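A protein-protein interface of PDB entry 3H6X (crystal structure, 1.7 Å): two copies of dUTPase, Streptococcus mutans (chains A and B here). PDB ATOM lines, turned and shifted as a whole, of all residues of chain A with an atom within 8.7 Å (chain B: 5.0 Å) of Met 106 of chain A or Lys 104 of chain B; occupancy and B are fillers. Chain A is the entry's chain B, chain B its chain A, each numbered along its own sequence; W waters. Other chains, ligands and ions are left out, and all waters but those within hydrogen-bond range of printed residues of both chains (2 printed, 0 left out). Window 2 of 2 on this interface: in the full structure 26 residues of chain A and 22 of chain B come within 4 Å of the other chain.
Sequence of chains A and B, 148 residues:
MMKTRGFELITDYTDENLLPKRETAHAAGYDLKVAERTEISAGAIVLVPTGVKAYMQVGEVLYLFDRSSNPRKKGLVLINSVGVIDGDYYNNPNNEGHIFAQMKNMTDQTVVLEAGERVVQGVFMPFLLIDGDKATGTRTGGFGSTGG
Ile 45 of chain B touches Pro 71 of chain A (CD1 to O, 3.9997 Å). O of Ile 79 of chain B touches CG of Pro 71 of chain A (3.7 Å). Pro 71 of chain A touches Gln 102 of chain B. CG1 of Val 77 of chain A touches O of Ile 79 of chain B, at 3.6 Å. Ile 79 of chain B touches Met 106 of chain A. NZ of Lys 104 of chain B touches SD of Met 106 of chain A, 3.9 Å away.
N of Arg 72 of chain A sits close to NE2 of Gln 102 of chain B (3.4 Å).
N of Met 106 of chain A is in hydrogen-bond range of O of Gly 75 of chain A, at 2.9 Å. The backbone carbonyl oxygen (O) of Val 77 of chain A is in hydrogen-bond range of the backbone NH (N) of Lys 104 of chain A (2.9 Å). The backbone carbonyl oxygen (O) of Val 77 of chain B is in hydrogen-bond range of the backbone NH (N) of Lys 104 of chain B (2.8 Å). The backbone NH of Ile 79 of chain B lies within hydrogen-bond range of the backbone carbonyl oxygen of Gln 102 of chain B, 2.9 Å away.
Hydrophobic or aromatic side chains of chain B within 4 Å of the printed part of chain A: Ile 45 and Ile 79. Printed residues of chain A that touch a printed residue of chain B: Pro 71, Arg 72, Val 77 and Met 106. Among the printed residues, 7 pairs touch across the chains.
Water W2 lies within hydrogen-bond range of the side-chain carboxylate (OD2) of Asp 66 of chain A and the backbone carbonyl oxygen (O) of Ile 79 of chain B. Water W1 bridges NZ of Lys 104 of chain B (2.9 Å) and SD of Met 106 of chain A (3.2 Å).
Val 77 of chain A touches Ile 79 of chain B, but with the chains exchanged Ile 79 of chain A does not touch Val 77 of chain B (9.8 Å). Met 106 of chain A touches Ile 79 of chain B, but with the chains exchanged Ile 79 of chain A does not touch Met 106 of chain B (10.2 Å). Met 106 of chain A touches Lys 104 of chain B, but with the chains exchanged Lys 104 of chain A does not touch Met 106 of chain B (10.3 Å). Positions printed for both chains: 40, 43, 44, 45, 75, 76, 77, 79, 103, 104, 105 and 106. Of the 7 pairs that touch across the chains among the printed residues, none has its exchanged pair printed and touching as well.
Printed residues of chain B within 4 Å of Arg 72 of chain A: Gln 102 (3.3 Å). Gly 75 of chain A touches none of the printed residues of chain B. Printed residues of chain B within 4 Å of Met 106 of chain A: Ile 79 (3.99 Å) and Lys 104 (3.9 Å). Of the printed residues of chain A, Gln 102 of chain B touches Pro 71 and Arg 72. The nearest printed residue of chain B that does not touch Met 106 of chain A is Ile 45 of chain B (4.3 Å). The nearest printed residue of chain A that does not touch Ile 45 of chain B is Arg 72 of chain A (4.2 Å).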
ATOM      1  N   ILE A  40      -7.336   9.518  -8.195  1.00  0.00           N
ATOM      2  CA  ILE A  40      -6.297   9.383  -9.206  1.00  0.00           C
ATOM      3  C   ILE A  40      -6.663   8.248 -10.156  1.00  0.00           C
ATOM      4  O   ILE A  40      -6.676   7.078  -9.760  1.00  0.00           O
ATOM      5  CB  ILE A  40      -4.908   9.118  -8.585  1.00  0.00           C
ATOM      6  CG1 ILE A  40      -4.625  10.155  -7.482  1.00  0.00           C
ATOM      7  CG2 ILE A  40      -3.851   9.178  -9.658  1.00  0.00           C
ATOM      8  CD1 ILE A  40      -3.279  10.002  -6.816  1.00  0.00           C
ATOM      9  N   SER A  41      -6.986   8.611 -11.394  1.00  0.00           N
ATOM     10  CA  SER A  41      -7.353   7.633 -12.413  1.00  0.00           C
ATOM     11  C   SER A  41      -6.227   6.650 -12.721  1.00  0.00           C
ATOM     12  O   SER A  41      -5.055   6.914 -12.487  1.00  0.00           O
ATOM     13  CB  SER A  41      -7.786   8.338 -13.706  1.00  0.00           C
ATOM     14  OG  SER A  41      -8.868   9.210 -13.442  1.00  0.00           O
ATOM     15  N   ALA A  42      -6.595   5.498 -13.265  1.00  0.00           N
ATOM     16  CA  ALA A  42      -5.610   4.516 -13.698  1.00  0.00           C
ATOM     17  C   ALA A  42      -4.534   5.136 -14.574  1.00  0.00           C
ATOM     18  O   ALA A  42      -4.836   5.790 -15.582  1.00  0.00           O
ATOM     19  CB  ALA A  42      -6.312   3.368 -14.453  1.00  0.00           C
ATOM     20  N   GLY A  43      -3.274   4.939 -14.179  1.00  0.00           N
ATOM     21  CA  GLY A  43      -2.147   5.453 -14.937  1.00  0.00           C
ATOM     22  C   GLY A  43      -1.904   6.956 -14.896  1.00  0.00           C
ATOM     23  O   GLY A  43      -0.946   7.445 -15.516  1.00  0.00           O
ATOM     24  N   ALA A  44      -2.743   7.690 -14.172  1.00  0.00           N
ATOM     25  CA  ALA A  44      -2.668   9.162 -14.166  1.00  0.00           C
ATOM     26  C   ALA A  44      -1.684   9.712 -13.135  1.00  0.00           C
ATOM     27  O   ALA A  44      -1.394   9.068 -12.120  1.00  0.00           O
ATOM     28  CB  ALA A  44      -4.032   9.754 -13.927  1.00  0.00           C
ATOM     29  N   ILE A  45      -1.219  10.932 -13.398  1.00  0.00           N
ATOM     30  CA  ILE A  45      -0.425  11.691 -12.433  1.00  0.00           C
ATOM     31  C   ILE A  45      -1.279  12.845 -11.906  1.00  0.00           C
ATOM     32  O   ILE A  45      -1.840  13.616 -12.697  1.00  0.00           O
ATOM     33  CB  ILE A  45       0.831  12.285 -13.069  1.00  0.00           C
ATOM     34  CG1 ILE A  45       1.766  11.186 -13.588  1.00  0.00           C
ATOM     35  CG2 ILE A  45       1.582  13.158 -12.036  1.00  0.00           C
ATOM     36  CD1 ILE A  45       2.892  11.707 -14.440  1.00  0.00           C
ATOM     37  N   ASP A  66       8.497   9.342  -0.626  1.00  0.00           N
ATOM     38  CA  ASP A  66       7.360   8.447  -0.653  1.00  0.00           C
ATOM     39  C   ASP A  66       7.268   7.723   0.693  1.00  0.00           C
ATOM     40  O   ASP A  66       8.267   7.530   1.385  1.00  0.00           O
ATOM     41  CB  ASP A  66       7.604   7.377  -1.727  1.00  0.00           C
ATOM     42  CG  ASP A  66       6.409   7.164  -2.619  1.00  0.00           C
ATOM     43  OD1 ASP A  66       5.271   7.503  -2.205  1.00  0.00           O
ATOM     44  OD2 ASP A  66       6.612   6.701  -3.752  1.00  0.00           O
ATOM     45  N   SER A  69       4.809   2.226   2.186  1.00  0.00           N
ATOM     46  CA  SER A  69       3.633   1.417   1.843  1.00  0.00           C
ATOM     47  C   SER A  69       2.889   1.912   0.594  1.00  0.00           C
ATOM     48  O   SER A  69       2.028   1.214   0.068  1.00  0.00           O
ATOM     49  CB  SER A  69       2.665   1.354   3.016  1.00  0.00           C
ATOM     50  OG  SER A  69       2.188   2.647   3.335  1.00  0.00           O
ATOM     51  N   ASN A  70       3.219   3.102   0.094  1.00  0.00           N
ATOM     52  CA  ASN A  70       2.467   3.621  -1.059  1.00  0.00           C
ATOM     53  C   ASN A  70       2.478   2.667  -2.266  1.00  0.00           C
ATOM     54  O   ASN A  70       1.422   2.309  -2.757  1.00  0.00           O
ATOM     55  CB  ASN A  70       2.944   5.006  -1.473  1.00  0.00           C
ATOM     56  CG  ASN A  70       2.380   6.100  -0.602  1.00  0.00           C
ATOM     57  OD1 ASN A  70       1.427   5.879   0.149  1.00  0.00           O
ATOM     58  ND2 ASN A  70       2.969   7.307  -0.702  1.00  0.00           N
ATOM     59  N   PRO A  71       3.667   2.224  -2.714  1.00  0.00           N
ATOM     60  CA  PRO A  71       3.631   1.408  -3.932  1.00  0.00           C
ATOM     61  C   PRO A  71       3.045   0.024  -3.719  1.00  0.00           C
ATOM     62  O   PRO A  71       2.203  -0.410  -4.499  1.00  0.00           O
ATOM     63  CB  PRO A  71       5.108   1.276  -4.338  1.00  0.00           C
ATOM     64  CG  PRO A  71       5.856   2.291  -3.548  1.00  0.00           C
ATOM     65  CD  PRO A  71       5.016   2.734  -2.396  1.00  0.00           C
ATOM     66  N   ARG A  72       3.497  -0.688  -2.695  1.00  0.00           N
ATOM     67  CA  ARG A  72       3.043  -2.071  -2.599  1.00  0.00           C
ATOM     68  C   ARG A  72       1.655  -2.223  -1.988  1.00  0.00           C
ATOM     69  O   ARG A  72       0.990  -3.217  -2.248  1.00  0.00           O
ATOM     70  CB  ARG A  72       4.079  -2.989  -1.943  1.00  0.00           C
ATOM     71  CG  ARG A  72       4.245  -2.844  -0.476  1.00  0.00           C
ATOM     72  CD  ARG A  72       5.130  -3.990   0.018  1.00  0.00           C
ATOM     73  NE  ARG A  72       5.507  -3.895   1.425  1.00  0.00           N
ATOM     74  CZ  ARG A  72       4.738  -3.405   2.394  1.00  0.00           C
ATOM     75  NH1 ARG A  72       3.515  -2.980   2.126  1.00  0.00           N
ATOM     76  NH2 ARG A  72       5.184  -3.365   3.643  1.00  0.00           N
ATOM     77  N   LYS A  73       1.194  -1.229  -1.227  1.00  0.00           N
ATOM     78  CA  LYS A  73      -0.140  -1.305  -0.649  1.00  0.00           C
ATOM     79  C   LYS A  73      -1.192  -0.532  -1.410  1.00  0.00           C
ATOM     80  O   LYS A  73      -2.322  -1.003  -1.533  1.00  0.00           O
ATOM     81  CB  LYS A  73      -0.123  -0.842   0.805  1.00  0.00           C
ATOM     82  CG  LYS A  73       0.828  -1.637   1.660  1.00  0.00           C
ATOM     83  CD  LYS A  73       0.128  -2.848   2.188  1.00  0.00           C
ATOM     84  CE  LYS A  73      -0.655  -2.443   3.409  1.00  0.00           C
ATOM     85  NZ  LYS A  73      -1.997  -3.060   3.422  1.00  0.00           N
ATOM     86  N   LYS A  74      -0.835   0.651  -1.913  1.00  0.00           N
ATOM     87  CA  LYS A  74      -1.821   1.510  -2.564  1.00  0.00           C
ATOM     88  C   LYS A  74      -1.673   1.588  -4.075  1.00  0.00           C
ATOM     89  O   LYS A  74      -2.572   2.072  -4.765  1.00  0.00           O
ATOM     90  CB  LYS A  74      -1.761   2.931  -2.008  1.00  0.00           C
ATOM     91  CG  LYS A  74      -2.075   3.076  -0.543  1.00  0.00           C
ATOM     92  CD  LYS A  74      -2.110   4.545  -0.185  1.00  0.00           C
ATOM     93  CE  LYS A  74      -3.092   4.835   0.945  1.00  0.00           C
ATOM     94  NZ  LYS A  74      -2.552   4.409   2.249  1.00  0.00           N
ATOM     95  N   GLY A  75      -0.540   1.132  -4.594  1.00  0.00           N
ATOM     96  CA  GLY A  75      -0.301   1.194  -6.023  1.00  0.00           C
ATOM     97  C   GLY A  75       0.066   2.588  -6.494  1.00  0.00           C
ATOM     98  O   GLY A  75      -0.045   2.890  -7.680  1.00  0.00           O
ATOM     99  N   LEU A  76       0.538   3.424  -5.566  1.00  0.00           N
ATOM    100  CA  LEU A  76       0.891   4.817  -5.883  1.00  0.00           C
ATOM    101  C   LEU A  76       2.375   5.050  -5.661  1.00  0.00           C
ATOM    102  O   LEU A  76       2.961   4.478  -4.735  1.00  0.00           O
ATOM    103  CB  LEU A  76       0.145   5.786  -4.966  1.00  0.00           C
ATOM    104  CG  LEU A  76      -1.387   5.735  -4.946  1.00  0.00           C
ATOM    105  CD1 LEU A  76      -1.902   6.779  -3.973  1.00  0.00           C
ATOM    106  CD2 LEU A  76      -1.951   5.964  -6.361  1.00  0.00           C
ATOM    107  N   VAL A  77       2.972   5.898  -6.495  1.00  0.00           N
ATOM    108  CA  VAL A  77       4.358   6.329  -6.301  1.00  0.00           C
ATOM    109  C   VAL A  77       4.490   7.839  -6.444  1.00  0.00           C
ATOM    110  O   VAL A  77       3.743   8.469  -7.182  1.00  0.00           O
ATOM    111  CB  VAL A  77       5.340   5.652  -7.289  1.00  0.00           C
ATOM    112  CG1 VAL A  77       5.395   4.135  -7.051  1.00  0.00           C
ATOM    113  CG2 VAL A  77       4.976   5.976  -8.734  1.00  0.00           C
ATOM    114  N   LEU A  78       5.460   8.406  -5.729  1.00  0.00           N
ATOM    115  CA  LEU A  78       5.836   9.809  -5.906  1.00  0.00           C
ATOM    116  C   LEU A  78       6.642   9.879  -7.212  1.00  0.00           C
ATOM    117  O   LEU A  78       7.787   9.413  -7.261  1.00  0.00           O
ATOM    118  CB  LEU A  78       6.678  10.251  -4.706  1.00  0.00           C
ATOM    119  CG  LEU A  78       7.063  11.735  -4.670  1.00  0.00           C
ATOM    120  CD1 LEU A  78       5.836  12.613  -4.555  1.00  0.00           C
ATOM    121  CD2 LEU A  78       7.976  12.009  -3.503  1.00  0.00           C
ATOM    122  N   ILE A  79       6.032  10.426  -8.266  1.00  0.00           N
ATOM    123  CA  ILE A  79       6.524  10.198  -9.617  1.00  0.00           C
ATOM    124  C   ILE A  79       7.833  10.923  -9.918  1.00  0.00           C
ATOM    125  O   ILE A  79       8.601  10.467 -10.773  1.00  0.00           O
ATOM    126  CB  ILE A  79       5.440  10.482 -10.684  1.00  0.00           C
ATOM    127  CG1 ILE A  79       5.805   9.838 -12.040  1.00  0.00           C
ATOM    128  CG2 ILE A  79       5.188  11.992 -10.791  1.00  0.00           C
ATOM    129  CD1 ILE A  79       6.028   8.320 -12.006  1.00  0.00           C
ATOM    130  N   MET A 103       1.679  12.365  -7.399  1.00  0.00           N
ATOM    131  CA  MET A 103       1.516  10.912  -7.243  1.00  0.00           C
ATOM    132  C   MET A 103       1.004  10.298  -8.545  1.00  0.00           C
ATOM    133  O   MET A 103       0.114  10.862  -9.196  1.00  0.00           O
ATOM    134  CB  MET A 103       0.525  10.606  -6.131  1.00  0.00           C
ATOM    135  CG  MET A 103       0.809  11.300  -4.816  1.00  0.00           C
ATOM    136  SD  MET A 103       2.518  10.721  -4.074  1.00  0.00           S
ATOM    137  CE  MET A 103       2.146   8.811  -3.908  1.00  0.00           C
ATOM    138  N   LYS A 104       1.576   9.155  -8.915  1.00  0.00           N
ATOM    139  CA  LYS A 104       1.114   8.404 -10.079  1.00  0.00           C
ATOM    140  C   LYS A 104       0.452   7.108  -9.638  1.00  0.00           C
ATOM    141  O   LYS A 104       0.958   6.398  -8.775  1.00  0.00           O
ATOM    142  CB  LYS A 104       2.269   8.080 -11.036  1.00  0.00           C
ATOM    143  CG  LYS A 104       1.782   7.283 -12.257  1.00  0.00           C
ATOM    144  CD  LYS A 104       2.847   7.160 -13.331  1.00  0.00           C
ATOM    145  CE  LYS A 104       2.377   6.217 -14.431  1.00  0.00           C
ATOM    146  NZ  LYS A 104       3.365   6.177 -15.558  1.00  0.00           N
ATOM    147  N   ASN A 105      -0.693   6.798 -10.245  1.00  0.00           N
ATOM    148  CA  ASN A 105      -1.379   5.539  -9.993  1.00  0.00           C
ATOM    149  C   ASN A 105      -0.884   4.503 -11.005  1.00  0.00           C
ATOM    150  O   ASN A 105      -1.184   4.601 -12.198  1.00  0.00           O
ATOM    151  CB  ASN A 105      -2.881   5.772 -10.141  1.00  0.00           C
ATOM    152  CG  ASN A 105      -3.710   4.507  -9.962  1.00  0.00           C
ATOM    153  OD1 ASN A 105      -3.184   3.412  -9.751  1.00  0.00           O
ATOM    154  ND2 ASN A 105      -5.029   4.662 -10.029  1.00  0.00           N
ATOM    155  N   MET A 106      -0.119   3.525 -10.516  1.00  0.00           N
ATOM    156  CA  MET A 106       0.450   2.480 -11.353  1.00  0.00           C
ATOM    157  C   MET A 106      -0.535   1.377 -11.721  1.00  0.00           C
ATOM    158  O   MET A 106      -0.219   0.541 -12.570  1.00  0.00           O
ATOM    159  CB  MET A 106       1.625   1.816 -10.646  1.00  0.00           C
ATOM    160  CG  MET A 106       2.737   2.746 -10.299  1.00  0.00           C
ATOM    161  SD  MET A 106       4.199   1.713  -9.449  1.00  0.00           S
ATOM    162  CE  MET A 106       3.281   1.065  -7.864  1.00  0.00           C
ATOM    163  N   THR A 107      -1.698   1.369 -11.086  1.00  0.00           N
ATOM    164  CA  THR A 107      -2.671   0.287 -11.272  1.00  0.00           C
ATOM    165  C   THR A 107      -3.684   0.574 -12.377  1.00  0.00           C
ATOM    166  O   THR A 107      -3.680   1.639 -12.981  1.00  0.00           O
ATOM    167  CB  THR A 107      -3.448  -0.008  -9.978  1.00  0.00           C
ATOM    168  OG1 THR A 107      -4.483   0.964  -9.789  1.00  0.00           O
ATOM    169  CG2 THR A 107      -2.513   0.004  -8.767  1.00  0.00           C
ATOM    170  N   ASP A 108      -4.584  -0.380 -12.603  1.00  0.00           N
ATOM    171  CA  ASP A 108      -5.602  -0.221 -13.636  1.00  0.00           C
ATOM    172  C   ASP A 108      -6.974   0.166 -13.092  1.00  0.00           C
ATOM    173  O   ASP A 108      -7.963   0.128 -13.830  1.00  0.00           O
ATOM    174  CB  ASP A 108      -5.705  -1.488 -14.510  1.00  0.00           C
ATOM    175  CG  ASP A 108      -6.155  -2.704 -13.725  1.00  0.00           C
ATOM    176  OD1 ASP A 108      -6.546  -2.555 -12.546  1.00  0.00           O
ATOM    177  OD2 ASP A 108      -6.122  -3.827 -14.285  1.00  0.00           O
ATOM    178  N   GLN A 109      -7.035   0.540 -11.812  1.00  0.00           N
ATOM    179  CA  GLN A 109      -8.281   1.004 -11.195  1.00  0.00           C
ATOM    180  C   GLN A 109      -8.049   2.349 -10.531  1.00  0.00           C
ATOM    181  O   GLN A 109      -6.967   2.596  -9.999  1.00  0.00           O
ATOM    182  CB  GLN A 109      -8.743   0.038 -10.121  1.00  0.00           C
ATOM    183  CG  GLN A 109      -8.900  -1.386 -10.585  1.00  0.00           C
ATOM    184  CD  GLN A 109     -10.319  -1.702 -11.032  1.00  0.00           C
ATOM    185  OE1 GLN A 109     -11.290  -1.228 -10.445  1.00  0.00           O
ATOM    186  NE2 GLN A 109     -10.442  -2.523 -12.063  1.00  0.00           N
ATOM    187  N   VAL A 111      -7.711   5.067  -7.869  1.00  0.00           N
ATOM    188  CA  VAL A 111      -7.377   5.036  -6.445  1.00  0.00           C
ATOM    189  C   VAL A 111      -7.859   6.337  -5.818  1.00  0.00           C
ATOM    190  O   VAL A 111      -7.680   7.404  -6.396  1.00  0.00           O
ATOM    191  CB  VAL A 111      -5.857   4.866  -6.216  1.00  0.00           C
ATOM    192  CG1 VAL A 111      -5.529   5.020  -4.737  1.00  0.00           C
ATOM    193  CG2 VAL A 111      -5.391   3.501  -6.730  1.00  0.00           C
ATOM    194  N   ILE B  40      12.208 -12.193  -8.436  1.00  0.00           N
ATOM    195  CA  ILE B  40      11.169 -11.183  -8.638  1.00  0.00           C
ATOM    196  C   ILE B  40      10.494 -11.407  -9.985  1.00  0.00           C
ATOM    197  O   ILE B  40      11.119 -11.260 -11.038  1.00  0.00           O
ATOM    198  CB  ILE B  40      11.742  -9.741  -8.568  1.00  0.00           C
ATOM    199  CG1 ILE B  40      12.629  -9.581  -7.319  1.00  0.00           C
ATOM    200  CG2 ILE B  40      10.587  -8.735  -8.573  1.00  0.00           C
ATOM    201  CD1 ILE B  40      13.218  -8.193  -7.132  1.00  0.00           C
ATOM    202  N   GLY B  43       7.044  -7.633 -13.516  1.00  0.00           N
ATOM    203  CA  GLY B  43       6.130  -6.597 -13.078  1.00  0.00           C
ATOM    204  C   GLY B  43       5.856  -6.569 -11.588  1.00  0.00           C
ATOM    205  O   GLY B  43       5.094  -5.719 -11.124  1.00  0.00           O
ATOM    206  N   ALA B  44       6.465  -7.487 -10.838  1.00  0.00           N
ATOM    207  CA  ALA B  44       6.165  -7.628  -9.407  1.00  0.00           C
ATOM    208  C   ALA B  44       7.025  -6.733  -8.519  1.00  0.00           C
ATOM    209  O   ALA B  44       8.131  -6.336  -8.902  1.00  0.00           O
ATOM    210  CB  ALA B  44       6.336  -9.081  -8.968  1.00  0.00           C
ATOM    211  N   ILE B  45       6.503  -6.443  -7.330  1.00  0.00           N
ATOM    212  CA  ILE B  45       7.269  -5.780  -6.278  1.00  0.00           C
ATOM    213  C   ILE B  45       7.604  -6.787  -5.185  1.00  0.00           C
ATOM    214  O   ILE B  45       6.720  -7.491  -4.688  1.00  0.00           O
ATOM    215  CB  ILE B  45       6.469  -4.615  -5.644  1.00  0.00           C
ATOM    216  CG1 ILE B  45       6.153  -3.551  -6.699  1.00  0.00           C
ATOM    217  CG2 ILE B  45       7.232  -4.026  -4.472  1.00  0.00           C
ATOM    218  CD1 ILE B  45       5.130  -2.509  -6.238  1.00  0.00           C
ATOM    219  N   GLY B  75      17.037  -4.147 -14.864  1.00  0.00           N
ATOM    220  CA  GLY B  75      15.618  -3.936 -15.064  1.00  0.00           C
ATOM    221  C   GLY B  75      14.869  -3.782 -13.756  1.00  0.00           C
ATOM    222  O   GLY B  75      13.653  -3.939 -13.730  1.00  0.00           O
ATOM    223  N   LEU B  76      15.589  -3.460 -12.679  1.00  0.00           N
ATOM    224  CA  LEU B  76      14.978  -3.302 -11.356  1.00  0.00           C
ATOM    225  C   LEU B  76      15.078  -1.859 -10.877  1.00  0.00           C
ATOM    226  O   LEU B  76      16.064  -1.164 -11.158  1.00  0.00           O
ATOM    227  CB  LEU B  76      15.697  -4.169 -10.322  1.00  0.00           C
ATOM    228  CG  LEU B  76      15.829  -5.663 -10.595  1.00  0.00           C
ATOM    229  CD1 LEU B  76      16.569  -6.304  -9.441  1.00  0.00           C
ATOM    230  CD2 LEU B  76      14.453  -6.287 -10.780  1.00  0.00           C
ATOM    231  N   VAL B  77      14.056  -1.420 -10.150  1.00  0.00           N
ATOM    232  CA  VAL B  77      14.094  -0.115  -9.494  1.00  0.00           C
ATOM    233  C   VAL B  77      13.636  -0.231  -8.041  1.00  0.00           C
ATOM    234  O   VAL B  77      12.834  -1.106  -7.688  1.00  0.00           O
ATOM    235  CB  VAL B  77      13.215   0.955 -10.202  1.00  0.00           C
ATOM    236  CG1 VAL B  77      13.727   1.215 -11.607  1.00  0.00           C
ATOM    237  CG2 VAL B  77      11.727   0.533 -10.218  1.00  0.00           C
ATOM    238  N   ILE B  79      11.240   0.918  -5.716  1.00  0.00           N
ATOM    239  CA  ILE B  79       9.936   1.411  -6.149  1.00  0.00           C
ATOM    240  C   ILE B  79       9.422   2.566  -5.289  1.00  0.00           C
ATOM    241  O   ILE B  79       8.628   3.380  -5.756  1.00  0.00           O
ATOM    242  CB  ILE B  79       8.898   0.258  -6.236  1.00  0.00           C
ATOM    243  CG1 ILE B  79       7.675   0.685  -7.084  1.00  0.00           C
ATOM    244  CG2 ILE B  79       8.500  -0.213  -4.840  1.00  0.00           C
ATOM    245  CD1 ILE B  79       8.027   1.119  -8.509  1.00  0.00           C
ATOM    246  N   GLN B 102      12.638  -2.528  -1.299  1.00  0.00           N
ATOM    247  CA  GLN B 102      11.416  -2.778  -2.052  1.00  0.00           C
ATOM    248  C   GLN B 102      11.684  -2.601  -3.543  1.00  0.00           C
ATOM    249  O   GLN B 102      11.697  -1.473  -4.053  1.00  0.00           O
ATOM    250  CB  GLN B 102      10.323  -1.812  -1.582  1.00  0.00           C
ATOM    251  CG  GLN B 102       8.923  -2.236  -1.935  1.00  0.00           C
ATOM    252  CD  GLN B 102       7.882  -1.231  -1.476  1.00  0.00           C
ATOM    253  OE1 GLN B 102       8.051  -0.562  -0.448  1.00  0.00           O
ATOM    254  NE2 GLN B 102       6.808  -1.100  -2.244  1.00  0.00           N
ATOM    255  N   MET B 103      11.908  -3.716  -4.244  1.00  0.00           N
ATOM    256  CA  MET B 103      12.346  -3.646  -5.638  1.00  0.00           C
ATOM    257  C   MET B 103      11.229  -4.070  -6.579  1.00  0.00           C
ATOM    258  O   MET B 103      10.536  -5.064  -6.320  1.00  0.00           O
ATOM    259  CB  MET B 103      13.565  -4.544  -5.850  1.00  0.00           C
ATOM    260  CG  MET B 103      14.694  -4.308  -4.884  1.00  0.00           C
ATOM    261  SD  MET B 103      15.447  -2.486  -5.069  1.00  0.00           S
ATOM    262  CE  MET B 103      16.012  -2.563  -6.948  1.00  0.00           C
ATOM    263  N   LYS B 104      11.065  -3.331  -7.677  1.00  0.00           N
ATOM    264  CA  LYS B 104      10.128  -3.711  -8.729  1.00  0.00           C
ATOM    265  C   LYS B 104      10.870  -4.168  -9.975  1.00  0.00           C
ATOM    266  O   LYS B 104      11.826  -3.537 -10.402  1.00  0.00           O
ATOM    267  CB  LYS B 104       9.209  -2.540  -9.095  1.00  0.00           C
ATOM    268  CG  LYS B 104       8.194  -2.926 -10.193  1.00  0.00           C
ATOM    269  CD  LYS B 104       7.138  -1.855 -10.405  1.00  0.00           C
ATOM    270  CE  LYS B 104       6.291  -2.185 -11.618  1.00  0.00           C
ATOM    271  NZ  LYS B 104       5.144  -1.243 -11.742  1.00  0.00           N
ATOM    272  N   ASN B 105      10.399  -5.264 -10.560  1.00  0.00           N
ATOM    273  CA  ASN B 105      10.918  -5.744 -11.834  1.00  0.00           C
ATOM    274  C   ASN B 105      10.144  -5.111 -12.998  1.00  0.00           C
ATOM    275  O   ASN B 105       8.959  -5.419 -13.203  1.00  0.00           O
ATOM    276  CB  ASN B 105      10.796  -7.276 -11.850  1.00  0.00           C
ATOM    277  CG  ASN B 105      11.268  -7.900 -13.149  1.00  0.00           C
ATOM    278  OD1 ASN B 105      11.658  -7.213 -14.085  1.00  0.00           O
ATOM    279  ND2 ASN B 105      11.241  -9.230 -13.197  1.00  0.00           N
ATOM    280  N   MET B 106      10.804  -4.219 -13.746  1.00  0.00           N
ATOM    281  CA  MET B 106      10.148  -3.513 -14.844  1.00  0.00           C
ATOM    282  C   MET B 106      10.050  -4.336 -16.127  1.00  0.00           C
ATOM    283  O   MET B 106       9.389  -3.930 -17.079  1.00  0.00           O
ATOM    284  CB  MET B 106      10.882  -2.218 -15.167  1.00  0.00           C
ATOM    285  CG  MET B 106      11.017  -1.304 -14.000  1.00  0.00           C
ATOM    286  SD  MET B 106      11.848   0.323 -14.671  1.00  0.00           S
ATOM    287  CE  MET B 106      13.650  -0.361 -15.025  1.00  0.00           C
HETATM  288  O   HOH W   1       6.076   1.490 -12.016  1.00  0.00           O
HETATM  289  O   HOH W   2       8.542   6.270  -5.498  1.00  0.00           O
